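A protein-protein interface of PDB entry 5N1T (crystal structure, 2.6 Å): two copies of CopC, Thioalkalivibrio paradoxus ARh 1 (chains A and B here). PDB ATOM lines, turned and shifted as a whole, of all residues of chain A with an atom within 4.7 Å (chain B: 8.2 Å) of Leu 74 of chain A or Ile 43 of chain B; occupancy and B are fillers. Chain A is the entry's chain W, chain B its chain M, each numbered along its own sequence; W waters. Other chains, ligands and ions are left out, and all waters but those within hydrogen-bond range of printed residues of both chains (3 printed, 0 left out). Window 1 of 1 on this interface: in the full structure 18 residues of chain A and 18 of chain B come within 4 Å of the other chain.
The backbone NH (N) of Leu 74 of chain A is in hydrogen-bond range of the side-chain carboxylate (OD2) of Asp 45 of chain B (3.1 Å).
O of Ile 79 of chain B is in hydrogen-bond range of N of Ile 43 of chain A (2.8 Å).
The backbone carbonyl oxygen of Ile 79 of chain A is in hydrogen-bond range of the backbone NH of Ile 43 of chain B (2.7 Å).
Hydrophobic or aromatic side chains of chain B within 4 Å of the printed part of chain A: Ala 42, Ile 43, Val 44 and Ile 79.
Of the 11 printed residues of chain A, 6 touch a printed residue of chain B.
Printed residues of chain A that touch a printed residue of chain B: Ile 43, Leu 72, Ser 73, Leu 74, Gly 78 and Ile 79.
Among the printed residues, 11 pairs touch across the chains.
Ile 43 of chain A touches Ile 43 of chain B (CD1 to CD1, 3.9 Å).
Asp 45 of chain B touches Leu 72 of chain A (OD2 to O, 3.5 Å).
OD2 of Asp 45 of chain B touches CA of Ser 73 of chain A, 3.4 Å away.
CD1 of Leu 74 of chain A touches CG2 of Ile 43 of chain B (3.7 Å).
Val 44 of chain B touches Leu 74 of chain A.
O of Ile 43 of chain B touches CA of Gly 78 of chain A, at 3.0 Å.
CG1 of Val 44 of chain B touches CA of Gly 78 of chain A (3.6 Å).
Ala 42 of chain B touches Ile 79 of chain A.
The backbone carbonyl oxygen (O) of Ala 42 of chain B is in hydrogen-bond range of the backbone NH (N) of Val 151 of chain B (3.1 Å).
The backbone carbonyl oxygen (O) of Val 44 of chain B sits at hydrogen-bond distance from the backbone NH (N) of Ala 153 of chain B.
The backbone carbonyl oxygen (O) of Ala 129 of chain A lies within hydrogen-bond range of the backbone NH (N) of Leu 72 of chain A, 2.6 Å away.
The backbone carbonyl oxygen (O) of Val 151 of chain B sits at hydrogen-bond distance from the backbone NH (N) of Val 44 of chain B (2.8 Å).
Water W2 lies within hydrogen-bond range of the backbone carbonyl oxygen (O) of Leu 72 of chain A (2.5 Å), the side-chain carboxylate (OD1) of Asp 45 of chain B (2.8 Å) and the backbone NH (N) of Ala 129 of chain A (2.8 Å).
Water W3 lies within hydrogen-bond range of the backbone carbonyl oxygen of Pro 75 of chain A (2.7 Å) and the backbone NH of Asp 45 of chain B (2.8 Å).
Water W1 lies within hydrogen-bond range of O of Asp 45 of chain B and OE2 of Glu 76 of chain A.
Ile 43 of chain A touches its own counterpart, Ile 43 of chain B.
Ile 43 of chain A touches Ile 79 of chain B, and with the chains exchanged Ile 79 of chain A touches Ile 43 of chain B.
Of the printed residues of chain B, Leu 72 of chain A touches Asp 45.
Printed residues of chain B within 4 Å of Leu 74 of chain A: Ile 43, Val 44 and Asp 45.
Pro 75 of chain A touches none of the printed residues of chain B.
Printed residues of chain B within 4 Å of Gly 78 of chain A: Ile 43 and Val 44.
Ile 43 of chain B touches four residues of chain A.
Ala 149 of chain B touches none of the printed residues of chain A.
Ala 153 of chain B touches none of the printed residues of chain A.
The nearest residue of chain B that does not touch Leu 74 of chain A is Ala 153 of chain B (4.4 Å).
The nearest residue of chain A that does not touch Ile 43 of chain B is Val 151 of chain A (4.2 Å).
The nearest printed residue of chain A that does not touch Ala 42 of chain B is Gly 78 of chain A (4.4 Å).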
ATOM      1  N   ILE A  43     -20.487 -28.393 -29.419  1.00  0.00           N
ATOM      2  CA  ILE A  43     -21.070 -29.639 -28.983  1.00  0.00           C
ATOM      3  C   ILE A  43     -21.126 -30.544 -30.181  1.00  0.00           C
ATOM      4  O   ILE A  43     -21.718 -30.178 -31.212  1.00  0.00           O
ATOM      5  CB  ILE A  43     -22.467 -29.445 -28.382  1.00  0.00           C
ATOM      6  CG1 ILE A  43     -22.443 -28.185 -27.497  1.00  0.00           C
ATOM      7  CG2 ILE A  43     -22.859 -30.712 -27.609  1.00  0.00           C
ATOM      8  CD1 ILE A  43     -23.761 -27.754 -26.899  1.00  0.00           C
ATOM      9  N   LEU A  72     -14.566 -32.155 -17.603  1.00  0.00           N
ATOM     10  CA  LEU A  72     -15.159 -31.166 -16.674  1.00  0.00           C
ATOM     11  C   LEU A  72     -16.389 -31.762 -15.975  1.00  0.00           C
ATOM     12  O   LEU A  72     -17.270 -32.324 -16.650  1.00  0.00           O
ATOM     13  CB  LEU A  72     -15.510 -29.840 -17.414  1.00  0.00           C
ATOM     14  CG  LEU A  72     -14.337 -29.066 -18.087  1.00  0.00           C
ATOM     15  CD1 LEU A  72     -14.791 -27.860 -18.920  1.00  0.00           C
ATOM     16  CD2 LEU A  72     -13.255 -28.690 -17.058  1.00  0.00           C
ATOM     17  N   SER A  73     -16.427 -31.696 -14.640  1.00  0.00           N
ATOM     18  CA  SER A  73     -17.639 -32.059 -13.904  1.00  0.00           C
ATOM     19  C   SER A  73     -18.480 -30.819 -13.730  1.00  0.00           C
ATOM     20  O   SER A  73     -18.169 -29.936 -12.912  1.00  0.00           O
ATOM     21  CB  SER A  73     -17.345 -32.749 -12.579  1.00  0.00           C
ATOM     22  OG  SER A  73     -16.296 -32.091 -11.941  1.00  0.00           O
ATOM     23  N   LEU A  74     -19.540 -30.766 -14.534  1.00  0.00           N
ATOM     24  CA  LEU A  74     -20.364 -29.579 -14.710  1.00  0.00           C
ATOM     25  C   LEU A  74     -21.135 -29.205 -13.432  1.00  0.00           C
ATOM     26  O   LEU A  74     -21.247 -30.018 -12.536  1.00  0.00           O
ATOM     27  CB  LEU A  74     -21.290 -29.767 -15.918  1.00  0.00           C
ATOM     28  CG  LEU A  74     -20.669 -29.923 -17.327  1.00  0.00           C
ATOM     29  CD1 LEU A  74     -21.731 -30.462 -18.279  1.00  0.00           C
ATOM     30  CD2 LEU A  74     -20.095 -28.614 -17.874  1.00  0.00           C
ATOM     31  N   PRO A  75     -21.603 -27.953 -13.304  1.00  0.00           N
ATOM     32  CA  PRO A  75     -22.487 -27.686 -12.162  1.00  0.00           C
ATOM     33  C   PRO A  75     -23.750 -28.538 -12.192  1.00  0.00           C
ATOM     34  O   PRO A  75     -24.186 -28.941 -13.265  1.00  0.00           O
ATOM     35  CB  PRO A  75     -22.873 -26.219 -12.366  1.00  0.00           C
ATOM     36  CG  PRO A  75     -22.411 -25.863 -13.754  1.00  0.00           C
ATOM     37  CD  PRO A  75     -21.208 -26.702 -13.962  1.00  0.00           C
ATOM     38  N   GLU A  76     -24.319 -28.813 -11.023  1.00  0.00           N
ATOM     39  CA  GLU A  76     -25.619 -29.513 -10.907  1.00  0.00           C
ATOM     40  C   GLU A  76     -26.726 -29.064 -11.851  1.00  0.00           C
ATOM     41  O   GLU A  76     -27.490 -29.898 -12.301  1.00  0.00           O
ATOM     42  CB  GLU A  76     -26.176 -29.449  -9.486  1.00  0.00           C
ATOM     43  CG  GLU A  76     -25.341 -30.197  -8.476  1.00  0.00           C
ATOM     44  CD  GLU A  76     -25.038 -31.582  -8.954  1.00  0.00           C
ATOM     45  OE1 GLU A  76     -23.846 -31.865  -9.181  1.00  0.00           O
ATOM     46  OE2 GLU A  76     -26.004 -32.358  -9.143  1.00  0.00           O
ATOM     47  N   GLY A  78     -26.079 -27.268 -14.588  1.00  0.00           N
ATOM     48  CA  GLY A  78     -25.421 -27.231 -15.885  1.00  0.00           C
ATOM     49  C   GLY A  78     -25.053 -25.868 -16.422  1.00  0.00           C
ATOM     50  O   GLY A  78     -25.321 -24.838 -15.800  1.00  0.00           O
ATOM     51  N   ILE A  79     -24.466 -25.876 -17.612  1.00  0.00           N
ATOM     52  CA  ILE A  79     -24.117 -24.662 -18.295  1.00  0.00           C
ATOM     53  C   ILE A  79     -25.068 -24.447 -19.469  1.00  0.00           C
ATOM     54  O   ILE A  79     -25.703 -25.384 -19.939  1.00  0.00           O
ATOM     55  CB  ILE A  79     -22.625 -24.641 -18.714  1.00  0.00           C
ATOM     56  CG1 ILE A  79     -22.332 -25.673 -19.802  1.00  0.00           C
ATOM     57  CG2 ILE A  79     -21.698 -24.839 -17.509  1.00  0.00           C
ATOM     58  CD1 ILE A  79     -20.926 -25.564 -20.365  1.00  0.00           C
ATOM     59  N   LEU A  88     -15.336 -22.170 -16.894  1.00  0.00           N
ATOM     60  CA  LEU A  88     -15.136 -23.322 -16.048  1.00  0.00           C
ATOM     61  C   LEU A  88     -13.807 -23.972 -16.413  1.00  0.00           C
ATOM     62  O   LEU A  88     -13.004 -24.288 -15.523  1.00  0.00           O
ATOM     63  CB  LEU A  88     -16.335 -24.273 -16.179  1.00  0.00           C
ATOM     64  CG  LEU A  88     -16.407 -25.657 -15.532  1.00  0.00           C
ATOM     65  CD1 LEU A  88     -15.932 -25.629 -14.090  1.00  0.00           C
ATOM     66  CD2 LEU A  88     -17.832 -26.187 -15.614  1.00  0.00           C
ATOM     67  N   ALA A 129     -17.940 -32.643 -21.174  1.00  0.00           N
ATOM     68  CA  ALA A 129     -17.237 -31.388 -21.429  1.00  0.00           C
ATOM     69  C   ALA A 129     -15.771 -31.633 -21.096  1.00  0.00           C
ATOM     70  O   ALA A 129     -15.448 -32.139 -20.013  1.00  0.00           O
ATOM     71  CB  ALA A 129     -17.782 -30.276 -20.549  1.00  0.00           C
ATOM     72  N   VAL A 151     -17.547 -29.898 -26.013  1.00  0.00           N
ATOM     73  CA  VAL A 151     -18.459 -30.843 -25.378  1.00  0.00           C
ATOM     74  C   VAL A 151     -18.614 -32.031 -26.299  1.00  0.00           C
ATOM     75  O   VAL A 151     -19.059 -31.926 -27.464  1.00  0.00           O
ATOM     76  CB  VAL A 151     -19.845 -30.264 -25.048  1.00  0.00           C
ATOM     77  CG1 VAL A 151     -20.502 -31.149 -24.004  1.00  0.00           C
ATOM     78  CG2 VAL A 151     -19.760 -28.828 -24.546  1.00  0.00           C
ATOM     79  N   PRO B  39     -34.424 -32.954 -17.179  1.00  0.00           N
ATOM     80  CA  PRO B  39     -33.363 -31.969 -16.932  1.00  0.00           C
ATOM     81  C   PRO B  39     -33.646 -30.580 -17.512  1.00  0.00           C
ATOM     82  O   PRO B  39     -34.486 -30.449 -18.411  1.00  0.00           O
ATOM     83  CB  PRO B  39     -32.139 -32.604 -17.603  1.00  0.00           C
ATOM     84  CG  PRO B  39     -32.481 -34.045 -17.754  1.00  0.00           C
ATOM     85  CD  PRO B  39     -33.947 -34.028 -18.061  1.00  0.00           C
ATOM     86  N   PRO B  40     -32.977 -29.543 -16.973  1.00  0.00           N
ATOM     87  CA  PRO B  40     -33.241 -28.191 -17.452  1.00  0.00           C
ATOM     88  C   PRO B  40     -32.740 -28.033 -18.886  1.00  0.00           C
ATOM     89  O   PRO B  40     -31.908 -28.822 -19.338  1.00  0.00           O
ATOM     90  CB  PRO B  40     -32.394 -27.320 -16.508  1.00  0.00           C
ATOM     91  CG  PRO B  40     -31.278 -28.217 -16.042  1.00  0.00           C
ATOM     92  CD  PRO B  40     -31.938 -29.560 -15.912  1.00  0.00           C
ATOM     93  N   GLU B  41     -33.249 -27.031 -19.593  1.00  0.00           N
ATOM     94  CA  GLU B  41     -32.713 -26.678 -20.886  1.00  0.00           C
ATOM     95  C   GLU B  41     -31.281 -26.076 -20.742  1.00  0.00           C
ATOM     96  O   GLU B  41     -31.038 -24.859 -20.776  1.00  0.00           O
ATOM     97  CB  GLU B  41     -33.711 -25.788 -21.617  1.00  0.00           C
ATOM     98  CG  GLU B  41     -33.364 -25.542 -23.067  1.00  0.00           C
ATOM     99  CD  GLU B  41     -33.660 -24.112 -23.488  1.00  0.00           C
ATOM    100  OE1 GLU B  41     -33.012 -23.150 -22.957  1.00  0.00           O
ATOM    101  OE2 GLU B  41     -34.536 -23.967 -24.374  1.00  0.00           O
ATOM    102  N   ALA B  42     -30.323 -26.973 -20.582  1.00  0.00           N
ATOM    103  CA  ALA B  42     -28.925 -26.639 -20.335  1.00  0.00           C
ATOM    104  C   ALA B  42     -28.083 -27.850 -20.764  1.00  0.00           C
ATOM    105  O   ALA B  42     -28.657 -28.870 -21.159  1.00  0.00           O
ATOM    106  CB  ALA B  42     -28.748 -26.360 -18.846  1.00  0.00           C
ATOM    107  N   ILE B  43     -26.750 -27.755 -20.669  1.00  0.00           N
ATOM    108  CA  ILE B  43     -25.829 -28.905 -20.837  1.00  0.00           C
ATOM    109  C   ILE B  43     -25.561 -29.384 -19.447  1.00  0.00           C
ATOM    110  O   ILE B  43     -25.262 -28.568 -18.607  1.00  0.00           O
ATOM    111  CB  ILE B  43     -24.471 -28.477 -21.422  1.00  0.00           C
ATOM    112  CG1 ILE B  43     -24.644 -27.859 -22.808  1.00  0.00           C
ATOM    113  CG2 ILE B  43     -23.478 -29.640 -21.473  1.00  0.00           C
ATOM    114  CD1 ILE B  43     -23.515 -26.900 -23.125  1.00  0.00           C
ATOM    115  N   VAL B  44     -25.646 -30.688 -19.205  1.00  0.00           N
ATOM    116  CA  VAL B  44     -25.519 -31.256 -17.846  1.00  0.00           C
ATOM    117  C   VAL B  44     -24.806 -32.609 -17.774  1.00  0.00           C
ATOM    118  O   VAL B  44     -24.808 -33.360 -18.735  1.00  0.00           O
ATOM    119  CB  VAL B  44     -26.917 -31.437 -17.158  1.00  0.00           C
ATOM    120  CG1 VAL B  44     -27.422 -30.117 -16.650  1.00  0.00           C
ATOM    121  CG2 VAL B  44     -27.943 -32.098 -18.087  1.00  0.00           C
ATOM    122  N   ASP B  45     -24.258 -32.938 -16.612  1.00  0.00           N
ATOM    123  CA  ASP B  45     -23.764 -34.279 -16.341  1.00  0.00           C
ATOM    124  C   ASP B  45     -24.857 -35.166 -15.706  1.00  0.00           C
ATOM    125  O   ASP B  45     -24.923 -35.293 -14.456  1.00  0.00           O
ATOM    126  CB  ASP B  45     -22.555 -34.193 -15.399  1.00  0.00           C
ATOM    127  CG  ASP B  45     -21.276 -33.770 -16.104  1.00  0.00           C
ATOM    128  OD1 ASP B  45     -21.269 -33.607 -17.367  1.00  0.00           O
ATOM    129  OD2 ASP B  45     -20.266 -33.618 -15.366  1.00  0.00           O
ATOM    130  N   ALA B  46     -25.705 -35.774 -16.539  1.00  0.00           N
ATOM    131  CA  ALA B  46     -26.900 -36.489 -16.018  1.00  0.00           C
ATOM    132  C   ALA B  46     -26.686 -38.013 -15.973  1.00  0.00           C
ATOM    133  O   ALA B  46     -27.263 -38.767 -16.747  1.00  0.00           O
ATOM    134  CB  ALA B  46     -28.165 -36.096 -16.791  1.00  0.00           C
ATOM    135  N   ILE B  79     -22.606 -28.066 -32.864  1.00  0.00           N
ATOM    136  CA  ILE B  79     -23.447 -26.873 -32.575  1.00  0.00           C
ATOM    137  C   ILE B  79     -22.787 -25.979 -31.533  1.00  0.00           C
ATOM    138  O   ILE B  79     -22.164 -26.465 -30.570  1.00  0.00           O
ATOM    139  CB  ILE B  79     -24.924 -27.204 -32.185  1.00  0.00           C
ATOM    140  CG1 ILE B  79     -25.012 -28.064 -30.918  1.00  0.00           C
ATOM    141  CG2 ILE B  79     -25.655 -27.883 -33.335  1.00  0.00           C
ATOM    142  CD1 ILE B  79     -26.403 -28.166 -30.328  1.00  0.00           C
ATOM    143  N   ARG B  80     -22.917 -24.677 -31.753  1.00  0.00           N
ATOM    144  CA  ARG B  80     -22.177 -23.676 -30.983  1.00  0.00           C
ATOM    145  C   ARG B  80     -23.007 -23.060 -29.841  1.00  0.00           C
ATOM    146  O   ARG B  80     -22.475 -22.241 -29.083  1.00  0.00           O
ATOM    147  CB  ARG B  80     -21.599 -22.557 -31.901  1.00  0.00           C
ATOM    148  CG  ARG B  80     -20.470 -22.941 -32.869  1.00  0.00           C
ATOM    149  CD  ARG B  80     -19.660 -21.725 -33.345  1.00  0.00           C
ATOM    150  N   ASN B  81     -24.296 -23.412 -29.732  1.00  0.00           N
ATOM    151  CA  ASN B  81     -25.205 -22.803 -28.724  1.00  0.00           C
ATOM    152  C   ASN B  81     -26.606 -23.420 -28.667  1.00  0.00           C
ATOM    153  O   ASN B  81     -26.941 -24.265 -29.503  1.00  0.00           O
ATOM    154  CB  ASN B  81     -25.264 -21.247 -28.830  1.00  0.00           C
ATOM    155  CG  ASN B  81     -26.133 -20.750 -29.975  1.00  0.00           C
ATOM    156  OD1 ASN B  81     -27.222 -20.250 -29.738  1.00  0.00           O
ATOM    157  ND2 ASN B  81     -25.651 -20.863 -31.211  1.00  0.00           N
ATOM    158  N   LEU B  82     -27.401 -23.001 -27.669  1.00  0.00           N
ATOM    159  CA  LEU B  82     -28.761 -23.540 -27.427  1.00  0.00           C
ATOM    160  C   LEU B  82     -29.843 -23.166 -28.458  1.00  0.00           C
ATOM    161  O   LEU B  82     -30.719 -23.985 -28.717  1.00  0.00           O
ATOM    162  CB  LEU B  82     -29.261 -23.233 -26.013  1.00  0.00           C
ATOM    163  CG  LEU B  82     -28.559 -23.799 -24.767  1.00  0.00           C
ATOM    164  CD1 LEU B  82     -29.357 -23.341 -23.565  1.00  0.00           C
ATOM    165  CD2 LEU B  82     -28.356 -25.310 -24.720  1.00  0.00           C
ATOM    166  N   LEU B  85     -29.579 -25.767 -30.914  1.00  0.00           N
ATOM    167  CA  LEU B  85     -30.147 -27.023 -30.417  1.00  0.00           C
ATOM    168  C   LEU B  85     -31.665 -26.966 -30.551  1.00  0.00           C
ATOM    169  O   LEU B  85     -32.274 -27.932 -30.973  1.00  0.00           O
ATOM    170  CB  LEU B  85     -29.742 -27.258 -28.972  1.00  0.00           C
ATOM    171  CG  LEU B  85     -30.352 -28.425 -28.227  1.00  0.00           C
ATOM    172  CD1 LEU B  85     -29.693 -29.763 -28.526  1.00  0.00           C
ATOM    173  CD2 LEU B  85     -30.236 -28.095 -26.758  1.00  0.00           C
ATOM    174  N   GLY B 128     -26.097 -37.657 -24.897  1.00  0.00           N
ATOM    175  CA  GLY B 128     -26.566 -37.034 -26.134  1.00  0.00           C
ATOM    176  C   GLY B 128     -27.264 -35.687 -26.013  1.00  0.00           C
ATOM    177  O   GLY B 128     -27.686 -35.278 -24.924  1.00  0.00           O
ATOM    178  N   ALA B 149     -35.526 -29.248 -25.356  1.00  0.00           N
ATOM    179  CA  ALA B 149     -34.242 -29.904 -25.709  1.00  0.00           C
ATOM    180  C   ALA B 149     -33.236 -29.715 -24.602  1.00  0.00           C
ATOM    181  O   ALA B 149     -33.302 -28.742 -23.873  1.00  0.00           O
ATOM    182  CB  ALA B 149     -33.698 -29.335 -26.992  1.00  0.00           C
ATOM    183  N   PHE B 150     -32.318 -30.654 -24.468  1.00  0.00           N
ATOM    184  CA  PHE B 150     -31.237 -30.570 -23.481  1.00  0.00           C
ATOM    185  C   PHE B 150     -29.992 -31.332 -23.956  1.00  0.00           C
ATOM    186  O   PHE B 150     -30.054 -32.068 -24.941  1.00  0.00           O
ATOM    187  CB  PHE B 150     -31.703 -31.048 -22.096  1.00  0.00           C
ATOM    188  CG  PHE B 150     -32.083 -32.510 -22.018  1.00  0.00           C
ATOM    189  CD1 PHE B 150     -33.404 -32.932 -22.279  1.00  0.00           C
ATOM    190  CD2 PHE B 150     -31.146 -33.478 -21.604  1.00  0.00           C
ATOM    191  CE1 PHE B 150     -33.771 -34.283 -22.166  1.00  0.00           C
ATOM    192  CE2 PHE B 150     -31.514 -34.829 -21.501  1.00  0.00           C
ATOM    193  CZ  PHE B 150     -32.828 -35.233 -21.785  1.00  0.00           C
ATOM    194  N   VAL B 151     -28.863 -31.144 -23.272  1.00  0.00           N
ATOM    195  CA  VAL B 151     -27.682 -31.935 -23.554  1.00  0.00           C
ATOM    196  C   VAL B 151     -27.206 -32.681 -22.317  1.00  0.00           C
ATOM    197  O   VAL B 151     -26.933 -32.070 -21.286  1.00  0.00           O
ATOM    198  CB  VAL B 151     -26.577 -31.112 -24.215  1.00  0.00           C
ATOM    199  CG1 VAL B 151     -25.476 -32.030 -24.719  1.00  0.00           C
ATOM    200  CG2 VAL B 151     -27.148 -30.311 -25.375  1.00  0.00           C
ATOM    201  N   HIS B 152     -27.164 -34.010 -22.443  1.00  0.00           N
ATOM    202  CA  HIS B 152     -26.752 -34.963 -21.409  1.00  0.00           C
ATOM    203  C   HIS B 152     -25.374 -35.334 -21.861  1.00  0.00           C
ATOM    204  O   HIS B 152     -25.197 -35.853 -22.970  1.00  0.00           O
ATOM    205  CB  HIS B 152     -27.713 -36.189 -21.383  1.00  0.00           C
ATOM    206  CG  HIS B 152     -27.225 -37.395 -20.614  1.00  0.00           C
ATOM    207  ND1 HIS B 152     -26.163 -37.374 -19.731  1.00  0.00           N
ATOM    208  CD2 HIS B 152     -27.699 -38.666 -20.586  1.00  0.00           C
ATOM    209  CE1 HIS B 152     -25.990 -38.576 -19.216  1.00  0.00           C
ATOM    210  NE2 HIS B 152     -26.914 -39.378 -19.712  1.00  0.00           N
ATOM    211  N   ALA B 153     -24.394 -35.033 -21.022  1.00  0.00           N
ATOM    212  CA  ALA B 153     -23.004 -35.059 -21.432  1.00  0.00           C
ATOM    213  C   ALA B 153     -22.309 -36.202 -20.754  1.00  0.00           C
ATOM    214  O   ALA B 153     -21.102 -36.210 -20.688  1.00  0.00           O
ATOM    215  CB  ALA B 153     -22.325 -33.727 -21.102  1.00  0.00           C
ATOM    216  N   GLY B 154     -23.078 -37.164 -20.250  1.00  0.00           N
ATOM    217  CA  GLY B 154     -22.520 -38.358 -19.615  1.00  0.00           C
ATOM    218  C   GLY B 154     -22.209 -38.199 -18.150  1.00  0.00           C
ATOM    219  O   GLY B 154     -23.014 -37.646 -17.401  1.00  0.00           O
HETATM  220  O   HOH W   1     -25.039 -34.328 -11.548  1.00  0.00           O
HETATM  221  O   HOH W   2     -18.889 -32.687 -18.509  1.00  0.00           O
HETATM  222  O   HOH W   3     -24.221 -31.499 -14.167  1.00  0.00           O
